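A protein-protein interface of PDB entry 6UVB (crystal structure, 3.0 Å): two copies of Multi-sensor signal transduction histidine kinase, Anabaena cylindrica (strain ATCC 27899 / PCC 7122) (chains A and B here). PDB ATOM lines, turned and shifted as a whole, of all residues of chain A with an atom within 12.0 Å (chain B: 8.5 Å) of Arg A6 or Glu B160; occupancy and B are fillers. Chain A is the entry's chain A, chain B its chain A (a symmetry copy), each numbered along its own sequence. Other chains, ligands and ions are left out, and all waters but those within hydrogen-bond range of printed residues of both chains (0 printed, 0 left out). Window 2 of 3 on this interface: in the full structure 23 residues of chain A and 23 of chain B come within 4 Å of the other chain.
NE2 of Gln A3 sits close to OD2 of Asp B162. The guanidinium group of Arg A6 lies within salt-bridge range of the side-chain carboxylate of Glu B160 (3.6 Å). The guanidinium group (NH1) of Arg A6 lies within salt-bridge range of the side-chain carboxylate (OE2) of Glu B163 (3.97 Å).
Arg A6 touches just these residues of chain B: Glu B160 (2.3 Å) and Glu B163 (3.9 Å). Of the printed residues of chain A, Glu B160 touches Arg A6 (2.3 Å). No residue of chain A comes within 4 Å of Val B158. No residue of chain A comes within 4 Å of Trp B159. Glu B161 touches none of the printed residues of chain A. Of chain A, only Gln A3 (2.9 Å) comes within 4 Å of Asp B162. Of chain A, only Arg A6 comes within 4 Å of Glu B163. No residue of chain A comes within 4 Å of Ala B164. Printed residues of chain B within 4 Å of Gln A3: Asp B162. Of the printed residues of chain B, Ile A9 touches Leu B37 (3.5 Å). Of the printed residues of chain A, Leu B37 touches Ile A9. Gln A11 touches none of the printed residues of chain B. The nearest residue of chain B that does not touch Arg A6 is Asp B162 (4.3 Å).
Of the 17 printed residues of chain B, 5 touch a printed residue of chain A. Along chain B the printed residues that touch a printed residue of chain A span positions 37 to 166. Of the 16 printed residues of chain A, 4 touch a printed residue of chain B. Printed residues of chain A that touch a printed residue of chain B: Gln A3, Arg A6, Ile A9 and Ile A10. Hydrophobic or aromatic side chains of chain A that line the printed part of chain B: Ile A9 and Ile A10. Among the printed residues, Asp or Glu carboxylates within 4 Å of a Lys or Arg side-chain nitrogen of the other chain: Arg A6 with Glu B160 and Arg A6 with Glu B163.
Among the printed residues, pairs that only touch across the chains: Ile A9 with Leu B37 (3.5 Å) and Ile A10 with Leu B166 (3.8 Å).
The backbone carbonyl oxygen (O) of Ile A10 sits at hydrogen-bond distance from the side-chain hydroxyl (OG1) of Thr A14. OE2 of Glu B163 lies within salt-bridge range of NH1 of Arg B157 (2.9 Å). The backbone NH of Glu B160 sits at hydrogen-bond distance from the side-chain carboxylate of Glu B163. The side-chain amide oxygen of Gln B165 sits close to the side-chain carboxylate of Asp B162 (2.6 Å).
No position is printed for both chains.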
ATOM      1  N   MET A   1      29.243 -22.139  26.780  1.00  0.00           N
ATOM      2  CA  MET A   1      28.943 -21.716  25.424  1.00  0.00           C
ATOM      3  C   MET A   1      28.678 -20.211  25.401  1.00  0.00           C
ATOM      4  O   MET A   1      29.136 -19.465  26.271  1.00  0.00           O
ATOM      5  CB  MET A   1      27.741 -22.493  24.880  1.00  0.00           C
ATOM      6  CG  MET A   1      27.713 -22.612  23.369  1.00  0.00           C
ATOM      7  SD  MET A   1      29.167 -23.445  22.748  1.00  0.00           S
ATOM      8  CE  MET A   1      28.649 -25.153  22.873  1.00  0.00           C
ATOM      9  N   LEU A   2      27.946 -19.774  24.383  1.00  0.00           N
ATOM     10  CA  LEU A   2      27.496 -18.399  24.272  1.00  0.00           C
ATOM     11  C   LEU A   2      26.180 -18.173  24.997  1.00  0.00           C
ATOM     12  O   LEU A   2      25.589 -17.096  24.871  1.00  0.00           O
ATOM     13  CB  LEU A   2      27.367 -18.003  22.796  1.00  0.00           C
ATOM     14  CG  LEU A   2      27.636 -16.530  22.433  1.00  0.00           C
ATOM     15  CD1 LEU A   2      28.962 -16.059  23.010  1.00  0.00           C
ATOM     16  CD2 LEU A   2      27.596 -16.327  20.923  1.00  0.00           C
ATOM     17  N   GLN A   3      25.704 -19.166  25.752  1.00  0.00           N
ATOM     18  CA  GLN A   3      24.737 -18.899  26.811  1.00  0.00           C
ATOM     19  C   GLN A   3      25.241 -17.780  27.706  1.00  0.00           C
ATOM     20  O   GLN A   3      24.453 -17.158  28.429  1.00  0.00           O
ATOM     21  CB  GLN A   3      24.495 -20.190  27.616  1.00  0.00           C
ATOM     22  CG  GLN A   3      23.371 -20.162  28.645  1.00  0.00           C
ATOM     23  CD  GLN A   3      23.063 -21.543  29.228  1.00  0.00           C
ATOM     24  OE1 GLN A   3      23.232 -22.567  28.560  1.00  0.00           O
ATOM     25  NE2 GLN A   3      22.625 -21.571  30.485  1.00  0.00           N
ATOM     26  N   LEU A   4      26.560 -17.543  27.668  1.00  0.00           N
ATOM     27  CA  LEU A   4      27.190 -16.373  28.269  1.00  0.00           C
ATOM     28  C   LEU A   4      26.541 -15.071  27.806  1.00  0.00           C
ATOM     29  O   LEU A   4      26.289 -14.179  28.623  1.00  0.00           O
ATOM     30  CB  LEU A   4      28.686 -16.396  27.938  1.00  0.00           C
ATOM     31  CG  LEU A   4      29.521 -15.120  27.922  1.00  0.00           C
ATOM     32  CD1 LEU A   4      29.999 -14.714  29.314  1.00  0.00           C
ATOM     33  CD2 LEU A   4      30.702 -15.282  26.982  1.00  0.00           C
ATOM     34  N   GLN A   5      26.272 -14.929  26.505  1.00  0.00           N
ATOM     35  CA  GLN A   5      25.717 -13.670  26.011  1.00  0.00           C
ATOM     36  C   GLN A   5      24.248 -13.482  26.382  1.00  0.00           C
ATOM     37  O   GLN A   5      23.736 -12.359  26.268  1.00  0.00           O
ATOM     38  CB  GLN A   5      25.911 -13.565  24.488  1.00  0.00           C
ATOM     39  CG  GLN A   5      25.553 -12.200  23.851  1.00  0.00           C
ATOM     40  CD  GLN A   5      26.394 -11.030  24.370  1.00  0.00           C
ATOM     41  OE1 GLN A   5      25.865  -9.959  24.693  1.00  0.00           O
ATOM     42  NE2 GLN A   5      27.706 -11.224  24.431  1.00  0.00           N
ATOM     43  N   ARG A   6      23.565 -14.533  26.851  1.00  0.00           N
ATOM     44  CA  ARG A   6      22.202 -14.355  27.342  1.00  0.00           C
ATOM     45  C   ARG A   6      22.156 -13.350  28.490  1.00  0.00           C
ATOM     46  O   ARG A   6      21.265 -12.489  28.538  1.00  0.00           O
ATOM     47  CB  ARG A   6      21.620 -15.701  27.775  1.00  0.00           C
ATOM     48  CG  ARG A   6      21.498 -16.670  26.638  1.00  0.00           C
ATOM     49  CD  ARG A   6      20.323 -17.576  26.829  1.00  0.00           C
ATOM     50  NE  ARG A   6      20.095 -18.355  25.622  1.00  0.00           N
ATOM     51  CZ  ARG A   6      20.532 -19.594  25.443  1.00  0.00           C
ATOM     52  NH1 ARG A   6      20.285 -20.231  24.307  1.00  0.00           N
ATOM     53  NH2 ARG A   6      21.206 -20.197  26.403  1.00  0.00           N
ATOM     54  N   GLN A   7      23.130 -13.419  29.401  1.00  0.00           N
ATOM     55  CA  GLN A   7      23.092 -12.662  30.649  1.00  0.00           C
ATOM     56  C   GLN A   7      23.818 -11.318  30.592  1.00  0.00           C
ATOM     57  O   GLN A   7      23.791 -10.584  31.588  1.00  0.00           O
ATOM     58  CB  GLN A   7      23.685 -13.495  31.796  1.00  0.00           C
ATOM     59  CG  GLN A   7      23.286 -14.977  31.812  1.00  0.00           C
ATOM     60  CD  GLN A   7      23.345 -15.581  33.214  1.00  0.00           C
ATOM     61  OE1 GLN A   7      23.071 -14.893  34.204  1.00  0.00           O
ATOM     62  NE2 GLN A   7      23.696 -16.867  33.305  1.00  0.00           N
ATOM     63  N   LYS A   8      24.481 -10.982  29.482  1.00  0.00           N
ATOM     64  CA  LYS A   8      25.067  -9.653  29.325  1.00  0.00           C
ATOM     65  C   LYS A   8      24.043  -8.617  28.896  1.00  0.00           C
ATOM     66  O   LYS A   8      24.417  -7.467  28.646  1.00  0.00           O
ATOM     67  CB  LYS A   8      26.222  -9.666  28.316  1.00  0.00           C
ATOM     68  CG  LYS A   8      27.589 -10.009  28.907  1.00  0.00           C
ATOM     69  CD  LYS A   8      28.602 -10.279  27.799  1.00  0.00           C
ATOM     70  CE  LYS A   8      29.779 -11.110  28.295  1.00  0.00           C
ATOM     71  NZ  LYS A   8      30.504 -11.758  27.165  1.00  0.00           N
ATOM     72  N   ILE A   9      22.774  -9.007  28.781  1.00  0.00           N
ATOM     73  CA  ILE A   9      21.687  -8.053  28.685  1.00  0.00           C
ATOM     74  C   ILE A   9      20.703  -8.170  29.854  1.00  0.00           C
ATOM     75  O   ILE A   9      20.061  -7.173  30.201  1.00  0.00           O
ATOM     76  CB  ILE A   9      20.957  -8.190  27.333  1.00  0.00           C
ATOM     77  CG1 ILE A   9      19.838  -7.138  27.185  1.00  0.00           C
ATOM     78  CG2 ILE A   9      20.450  -9.610  27.168  1.00  0.00           C
ATOM     79  CD1 ILE A   9      20.309  -5.694  26.989  1.00  0.00           C
ATOM     80  N   ILE A  10      20.571  -9.352  30.479  1.00  0.00           N
ATOM     81  CA  ILE A  10      19.731  -9.446  31.679  1.00  0.00           C
ATOM     82  C   ILE A  10      20.284  -8.543  32.774  1.00  0.00           C
ATOM     83  O   ILE A  10      19.530  -7.887  33.505  1.00  0.00           O
ATOM     84  CB  ILE A  10      19.588 -10.909  32.159  1.00  0.00           C
ATOM     85  CG1 ILE A  10      18.330 -11.083  33.024  1.00  0.00           C
ATOM     86  CG2 ILE A  10      20.789 -11.355  32.987  1.00  0.00           C
ATOM     87  CD1 ILE A  10      18.532 -10.842  34.524  1.00  0.00           C
ATOM     88  N   GLN A  11      21.607  -8.479  32.890  1.00  0.00           N
ATOM     89  CA  GLN A  11      22.230  -7.507  33.767  1.00  0.00           C
ATOM     90  C   GLN A  11      22.075  -6.093  33.226  1.00  0.00           C
ATOM     91  O   GLN A  11      22.114  -5.138  34.011  1.00  0.00           O
ATOM     92  CB  GLN A  11      23.698  -7.891  33.972  1.00  0.00           C
ATOM     93  CG  GLN A  11      24.461  -6.996  34.918  1.00  0.00           C
ATOM     94  CD  GLN A  11      25.496  -6.178  34.192  1.00  0.00           C
ATOM     95  OE1 GLN A  11      26.202  -6.693  33.320  1.00  0.00           O
ATOM     96  NE2 GLN A  11      25.578  -4.888  34.523  1.00  0.00           N
ATOM     97  N   ASP A  12      21.878  -5.942  31.908  1.00  0.00           N
ATOM     98  CA  ASP A  12      21.478  -4.651  31.364  1.00  0.00           C
ATOM     99  C   ASP A  12      20.040  -4.343  31.729  1.00  0.00           C
ATOM    100  O   ASP A  12      19.738  -3.263  32.243  1.00  0.00           O
ATOM    101  CB  ASP A  12      21.624  -4.627  29.846  1.00  0.00           C
ATOM    102  CG  ASP A  12      23.052  -4.610  29.391  1.00  0.00           C
ATOM    103  OD1 ASP A  12      23.891  -4.016  30.098  1.00  0.00           O
ATOM    104  OD2 ASP A  12      23.336  -5.173  28.314  1.00  0.00           O
ATOM    105  N   ILE A  13      19.133  -5.272  31.435  1.00  0.00           N
ATOM    106  CA  ILE A  13      17.713  -4.982  31.602  1.00  0.00           C
ATOM    107  C   ILE A  13      17.390  -4.737  33.071  1.00  0.00           C
ATOM    108  O   ILE A  13      16.742  -3.739  33.423  1.00  0.00           O
ATOM    109  CB  ILE A  13      16.860  -6.108  30.995  1.00  0.00           C
ATOM    110  CG1 ILE A  13      17.098  -6.186  29.484  1.00  0.00           C
ATOM    111  CG2 ILE A  13      15.401  -5.871  31.279  1.00  0.00           C
ATOM    112  CD1 ILE A  13      16.283  -7.240  28.798  1.00  0.00           C
ATOM    113  N   THR A  14      17.873  -5.622  33.955  1.00  0.00           N
ATOM    114  CA  THR A  14      17.713  -5.388  35.388  1.00  0.00           C
ATOM    115  C   THR A  14      18.269  -4.031  35.777  1.00  0.00           C
ATOM    116  O   THR A  14      17.716  -3.348  36.643  1.00  0.00           O
ATOM    117  CB  THR A  14      18.414  -6.471  36.206  1.00  0.00           C
ATOM    118  OG1 THR A  14      18.046  -7.768  35.728  1.00  0.00           O
ATOM    119  CG2 THR A  14      18.030  -6.350  37.684  1.00  0.00           C
ATOM    120  N   GLN A  15      19.359  -3.626  35.126  1.00  0.00           N
ATOM    121  CA  GLN A  15      19.957  -2.325  35.393  1.00  0.00           C
ATOM    122  C   GLN A  15      18.976  -1.205  35.078  1.00  0.00           C
ATOM    123  O   GLN A  15      18.783  -0.293  35.889  1.00  0.00           O
ATOM    124  CB  GLN A  15      21.249  -2.168  34.583  1.00  0.00           C
ATOM    125  CG  GLN A  15      22.224  -1.157  35.143  1.00  0.00           C
ATOM    126  CD  GLN A  15      23.027  -1.724  36.289  1.00  0.00           C
ATOM    127  OE1 GLN A  15      23.671  -2.774  36.156  1.00  0.00           O
ATOM    128  NE2 GLN A  15      22.997  -1.035  37.429  1.00  0.00           N
ATOM    129  N   GLN A  16      18.334  -1.254  33.910  1.00  0.00           N
ATOM    130  CA  GLN A  16      17.420  -0.172  33.567  1.00  0.00           C
ATOM    131  C   GLN A  16      16.220  -0.133  34.499  1.00  0.00           C
ATOM    132  O   GLN A  16      15.696   0.955  34.792  1.00  0.00           O
ATOM    133  CB  GLN A  16      16.950  -0.302  32.123  1.00  0.00           C
ATOM    134  CG  GLN A  16      18.049  -0.084  31.111  1.00  0.00           C
ATOM    135  CD  GLN A  16      18.524  -1.376  30.514  1.00  0.00           C
ATOM    136  OE1 GLN A  16      17.721  -2.246  30.209  1.00  0.00           O
ATOM    137  NE2 GLN A  16      19.835  -1.528  30.365  1.00  0.00           N
ATOM    138  N   LEU B  37      16.524  -9.736  21.509  1.00  0.00           N
ATOM    139  CA  LEU B  37      17.542 -10.560  22.151  1.00  0.00           C
ATOM    140  C   LEU B  37      17.314 -12.046  21.893  1.00  0.00           C
ATOM    141  O   LEU B  37      18.269 -12.780  21.617  1.00  0.00           O
ATOM    142  CB  LEU B  37      17.568 -10.231  23.645  1.00  0.00           C
ATOM    143  CG  LEU B  37      17.683 -11.287  24.732  1.00  0.00           C
ATOM    144  CD1 LEU B  37      19.085 -11.888  24.786  1.00  0.00           C
ATOM    145  CD2 LEU B  37      17.320 -10.655  26.065  1.00  0.00           C
ATOM    146  N   MET B  38      16.063 -12.500  21.945  1.00  0.00           N
ATOM    147  CA  MET B  38      15.718 -13.893  21.697  1.00  0.00           C
ATOM    148  C   MET B  38      15.402 -14.189  20.232  1.00  0.00           C
ATOM    149  O   MET B  38      15.107 -15.347  19.904  1.00  0.00           O
ATOM    150  CB  MET B  38      14.533 -14.286  22.584  1.00  0.00           C
ATOM    151  CG  MET B  38      14.835 -14.141  24.079  1.00  0.00           C
ATOM    152  SD  MET B  38      13.621 -14.769  25.298  1.00  0.00           S
ATOM    153  CE  MET B  38      13.030 -16.298  24.536  1.00  0.00           C
ATOM    154  N   PRO B  91       7.590 -20.751  34.493  1.00  0.00           N
ATOM    155  CA  PRO B  91       7.134 -20.595  33.118  1.00  0.00           C
ATOM    156  C   PRO B  91       6.572 -21.863  32.523  1.00  0.00           C
ATOM    157  O   PRO B  91       6.416 -22.892  33.181  1.00  0.00           O
ATOM    158  CB  PRO B  91       8.397 -20.134  32.379  1.00  0.00           C
ATOM    159  CG  PRO B  91       9.466 -20.581  33.156  1.00  0.00           C
ATOM    160  CD  PRO B  91       9.032 -20.487  34.589  1.00  0.00           C
ATOM    161  N   ILE B  93       6.595 -24.014  28.656  1.00  0.00           N
ATOM    162  CA  ILE B  93       7.113 -24.108  27.301  1.00  0.00           C
ATOM    163  C   ILE B  93       6.097 -24.864  26.472  1.00  0.00           C
ATOM    164  O   ILE B  93       5.769 -26.020  26.770  1.00  0.00           O
ATOM    165  CB  ILE B  93       8.497 -24.770  27.237  1.00  0.00           C
ATOM    166  CG1 ILE B  93       9.519 -23.954  28.012  1.00  0.00           C
ATOM    167  CG2 ILE B  93       8.932 -24.895  25.781  1.00  0.00           C
ATOM    168  CD1 ILE B  93      10.890 -24.544  28.004  1.00  0.00           C
ATOM    169  N   ILE B 119       6.782 -19.520  24.619  1.00  0.00           N
ATOM    170  CA  ILE B 119       7.100 -19.604  26.032  1.00  0.00           C
ATOM    171  C   ILE B 119       6.227 -18.587  26.750  1.00  0.00           C
ATOM    172  O   ILE B 119       6.208 -17.410  26.378  1.00  0.00           O
ATOM    173  CB  ILE B 119       8.590 -19.332  26.301  1.00  0.00           C
ATOM    174  CG1 ILE B 119       9.461 -20.237  25.473  1.00  0.00           C
ATOM    175  CG2 ILE B 119       8.904 -19.574  27.704  1.00  0.00           C
ATOM    176  CD1 ILE B 119      10.841 -19.795  25.638  1.00  0.00           C
ATOM    177  N   ARG B 157      10.009 -23.715  16.746  1.00  0.00           N
ATOM    178  CA  ARG B 157      11.290 -23.532  17.401  1.00  0.00           C
ATOM    179  C   ARG B 157      11.394 -24.392  18.656  1.00  0.00           C
ATOM    180  O   ARG B 157      10.433 -24.541  19.427  1.00  0.00           O
ATOM    181  CB  ARG B 157      11.478 -22.060  17.754  1.00  0.00           C
ATOM    182  CG  ARG B 157      12.807 -21.766  18.339  1.00  0.00           C
ATOM    183  CD  ARG B 157      12.992 -20.302  18.443  1.00  0.00           C
ATOM    184  NE  ARG B 157      14.178 -19.982  19.207  1.00  0.00           N
ATOM    185  CZ  ARG B 157      14.527 -18.746  19.532  1.00  0.00           C
ATOM    186  NH1 ARG B 157      15.632 -18.537  20.237  1.00  0.00           N
ATOM    187  NH2 ARG B 157      13.769 -17.729  19.148  1.00  0.00           N
ATOM    188  N   VAL B 158      12.562 -24.954  18.864  1.00  0.00           N
ATOM    189  CA  VAL B 158      12.837 -25.635  20.117  1.00  0.00           C
ATOM    190  C   VAL B 158      13.469 -24.647  21.088  1.00  0.00           C
ATOM    191  O   VAL B 158      14.327 -23.829  20.721  1.00  0.00           O
ATOM    192  CB  VAL B 158      13.731 -26.857  19.886  1.00  0.00           C
ATOM    193  CG1 VAL B 158      12.927 -27.908  19.175  1.00  0.00           C
ATOM    194  CG2 VAL B 158      14.949 -26.450  19.076  1.00  0.00           C
ATOM    195  N   TRP B 159      13.032 -24.720  22.335  1.00  0.00           N
ATOM    196  CA  TRP B 159      13.457 -23.789  23.361  1.00  0.00           C
ATOM    197  C   TRP B 159      14.339 -24.505  24.385  1.00  0.00           C
ATOM    198  O   TRP B 159      14.155 -25.695  24.653  1.00  0.00           O
ATOM    199  CB  TRP B 159      12.236 -23.170  24.068  1.00  0.00           C
ATOM    200  CG  TRP B 159      11.172 -22.518  23.189  1.00  0.00           C
ATOM    201  CD1 TRP B 159       9.981 -23.064  22.775  1.00  0.00           C
ATOM    202  CD2 TRP B 159      11.198 -21.185  22.670  1.00  0.00           C
ATOM    203  NE1 TRP B 159       9.282 -22.153  22.016  1.00  0.00           N
ATOM    204  CE2 TRP B 159      10.006 -20.996  21.940  1.00  0.00           C
ATOM    205  CE3 TRP B 159      12.127 -20.141  22.742  1.00  0.00           C
ATOM    206  CZ2 TRP B 159       9.721 -19.813  21.301  1.00  0.00           C
ATOM    207  CZ3 TRP B 159      11.850 -18.975  22.122  1.00  0.00           C
ATOM    208  CH2 TRP B 159      10.662 -18.814  21.388  1.00  0.00           C
ATOM    209  N   GLU B 160      15.286 -23.766  24.967  1.00  0.00           N
ATOM    210  CA  GLU B 160      16.158 -24.267  26.019  1.00  0.00           C
ATOM    211  C   GLU B 160      15.594 -23.948  27.399  1.00  0.00           C
ATOM    212  O   GLU B 160      14.736 -23.083  27.545  1.00  0.00           O
ATOM    213  CB  GLU B 160      17.559 -23.668  25.889  1.00  0.00           C
ATOM    214  CG  GLU B 160      18.261 -24.024  24.607  1.00  0.00           C
ATOM    215  CD  GLU B 160      19.590 -23.317  24.458  1.00  0.00           C
ATOM    216  OE1 GLU B 160      19.650 -22.331  23.682  1.00  0.00           O
ATOM    217  OE2 GLU B 160      20.568 -23.756  25.115  1.00  0.00           O
ATOM    218  N   GLU B 161      16.100 -24.649  28.419  1.00  0.00           N
ATOM    219  CA  GLU B 161      15.689 -24.393  29.794  1.00  0.00           C
ATOM    220  C   GLU B 161      16.052 -22.983  30.197  1.00  0.00           C
ATOM    221  O   GLU B 161      15.270 -22.315  30.868  1.00  0.00           O
ATOM    222  CB  GLU B 161      16.336 -25.382  30.764  1.00  0.00           C
ATOM    223  CG  GLU B 161      17.414 -24.846  31.734  1.00  0.00           C
ATOM    224  CD  GLU B 161      17.553 -25.813  32.828  1.00  0.00           C
ATOM    225  OE1 GLU B 161      16.474 -26.089  33.384  1.00  0.00           O
ATOM    226  OE2 GLU B 161      18.642 -26.388  33.078  1.00  0.00           O
ATOM    227  N   ASP B 162      17.245 -22.542  29.813  1.00  0.00           N
ATOM    228  CA  ASP B 162      17.714 -21.231  30.209  1.00  0.00           C
ATOM    229  C   ASP B 162      17.129 -20.156  29.317  1.00  0.00           C
ATOM    230  O   ASP B 162      17.345 -18.970  29.572  1.00  0.00           O
ATOM    231  CB  ASP B 162      19.250 -21.209  30.209  1.00  0.00           C
ATOM    232  CG  ASP B 162      19.857 -22.392  30.981  1.00  0.00           C
ATOM    233  OD1 ASP B 162      19.907 -22.341  32.236  1.00  0.00           O
ATOM    234  OD2 ASP B 162      20.289 -23.363  30.324  1.00  0.00           O
ATOM    235  N   GLU B 163      16.371 -20.563  28.298  1.00  0.00           N
ATOM    236  CA  GLU B 163      15.580 -19.618  27.522  1.00  0.00           C
ATOM    237  C   GLU B 163      14.292 -19.279  28.259  1.00  0.00           C
ATOM    238  O   GLU B 163      13.955 -18.107  28.435  1.00  0.00           O
ATOM    239  CB  GLU B 163      15.307 -20.191  26.123  1.00  0.00           C
ATOM    240  CG  GLU B 163      16.431 -19.907  25.085  1.00  0.00           C
ATOM    241  CD  GLU B 163      16.055 -20.258  23.634  1.00  0.00           C
ATOM    242  OE1 GLU B 163      15.119 -21.054  23.439  1.00  0.00           O
ATOM    243  OE2 GLU B 163      16.696 -19.743  22.685  1.00  0.00           O
ATOM    244  N   ALA B 164      13.570 -20.296  28.713  1.00  0.00           N
ATOM    245  CA  ALA B 164      12.448 -20.056  29.612  1.00  0.00           C
ATOM    246  C   ALA B 164      12.914 -19.539  30.975  1.00  0.00           C
ATOM    247  O   ALA B 164      12.402 -18.517  31.447  1.00  0.00           O
ATOM    248  CB  ALA B 164      11.617 -21.319  29.761  1.00  0.00           C
ATOM    249  N   GLN B 165      13.873 -20.240  31.631  1.00  0.00           N
ATOM    250  CA  GLN B 165      14.526 -19.777  32.868  1.00  0.00           C
ATOM    251  C   GLN B 165      14.785 -18.271  32.692  1.00  0.00           C
ATOM    252  O   GLN B 165      14.461 -17.462  33.567  1.00  0.00           O
ATOM    253  CB  GLN B 165      15.805 -20.682  33.164  1.00  0.00           C
ATOM    254  CG  GLN B 165      16.955 -20.416  34.280  1.00  0.00           C
ATOM    255  CD  GLN B 165      17.716 -21.722  34.937  1.00  0.00           C
ATOM    256  OE1 GLN B 165      18.298 -22.658  34.290  1.00  0.00           O
ATOM    257  NE2 GLN B 165      17.641 -21.756  36.258  1.00  0.00           N
ATOM    258  N   LEU B 166      15.250 -17.855  31.508  1.00  0.00           N
ATOM    259  CA  LEU B 166      15.653 -16.448  31.324  1.00  0.00           C
ATOM    260  C   LEU B 166      14.454 -15.519  31.279  1.00  0.00           C
ATOM    261  O   LEU B 166      14.412 -14.497  31.987  1.00  0.00           O
ATOM    262  CB  LEU B 166      16.455 -16.277  30.035  1.00  0.00           C
ATOM    263  CG  LEU B 166      17.155 -14.982  29.605  1.00  0.00           C
ATOM    264  CD1 LEU B 166      16.307 -14.278  28.597  1.00  0.00           C
ATOM    265  CD2 LEU B 166      17.555 -14.026  30.754  1.00  0.00           C
ATOM    266  N   LEU B 167      13.476 -15.871  30.420  1.00  0.00           N
ATOM    267  CA  LEU B 167      12.201 -15.168  30.301  1.00  0.00           C
ATOM    268  C   LEU B 167      11.601 -14.863  31.667  1.00  0.00           C
ATOM    269  O   LEU B 167      11.414 -13.687  32.036  1.00  0.00           O
ATOM    270  CB  LEU B 167      11.223 -16.004  29.472  1.00  0.00           C
ATOM    271  CG  LEU B 167       9.996 -15.229  28.943  1.00  0.00           C
ATOM    272  CD1 LEU B 167      10.472 -14.078  28.135  1.00  0.00           C
ATOM    273  CD2 LEU B 167       9.072 -16.094  28.121  1.00  0.00           C
ATOM    274  N   ILE B 170      12.973 -12.200  33.637  1.00  0.00           N
ATOM    275  CA  ILE B 170      12.664 -10.865  33.143  1.00  0.00           C
ATOM    276  C   ILE B 170      11.260 -10.446  33.571  1.00  0.00           C
ATOM    277  O   ILE B 170      11.039  -9.291  33.967  1.00  0.00           O
ATOM    278  CB  ILE B 170      12.849 -10.828  31.613  1.00  0.00           C
ATOM    279  CG1 ILE B 170      14.318 -11.129  31.266  1.00  0.00           C
ATOM    280  CG2 ILE B 170      12.432  -9.453  31.024  1.00  0.00           C
ATOM    281  CD1 ILE B 170      14.612 -11.008  29.772  1.00  0.00           C
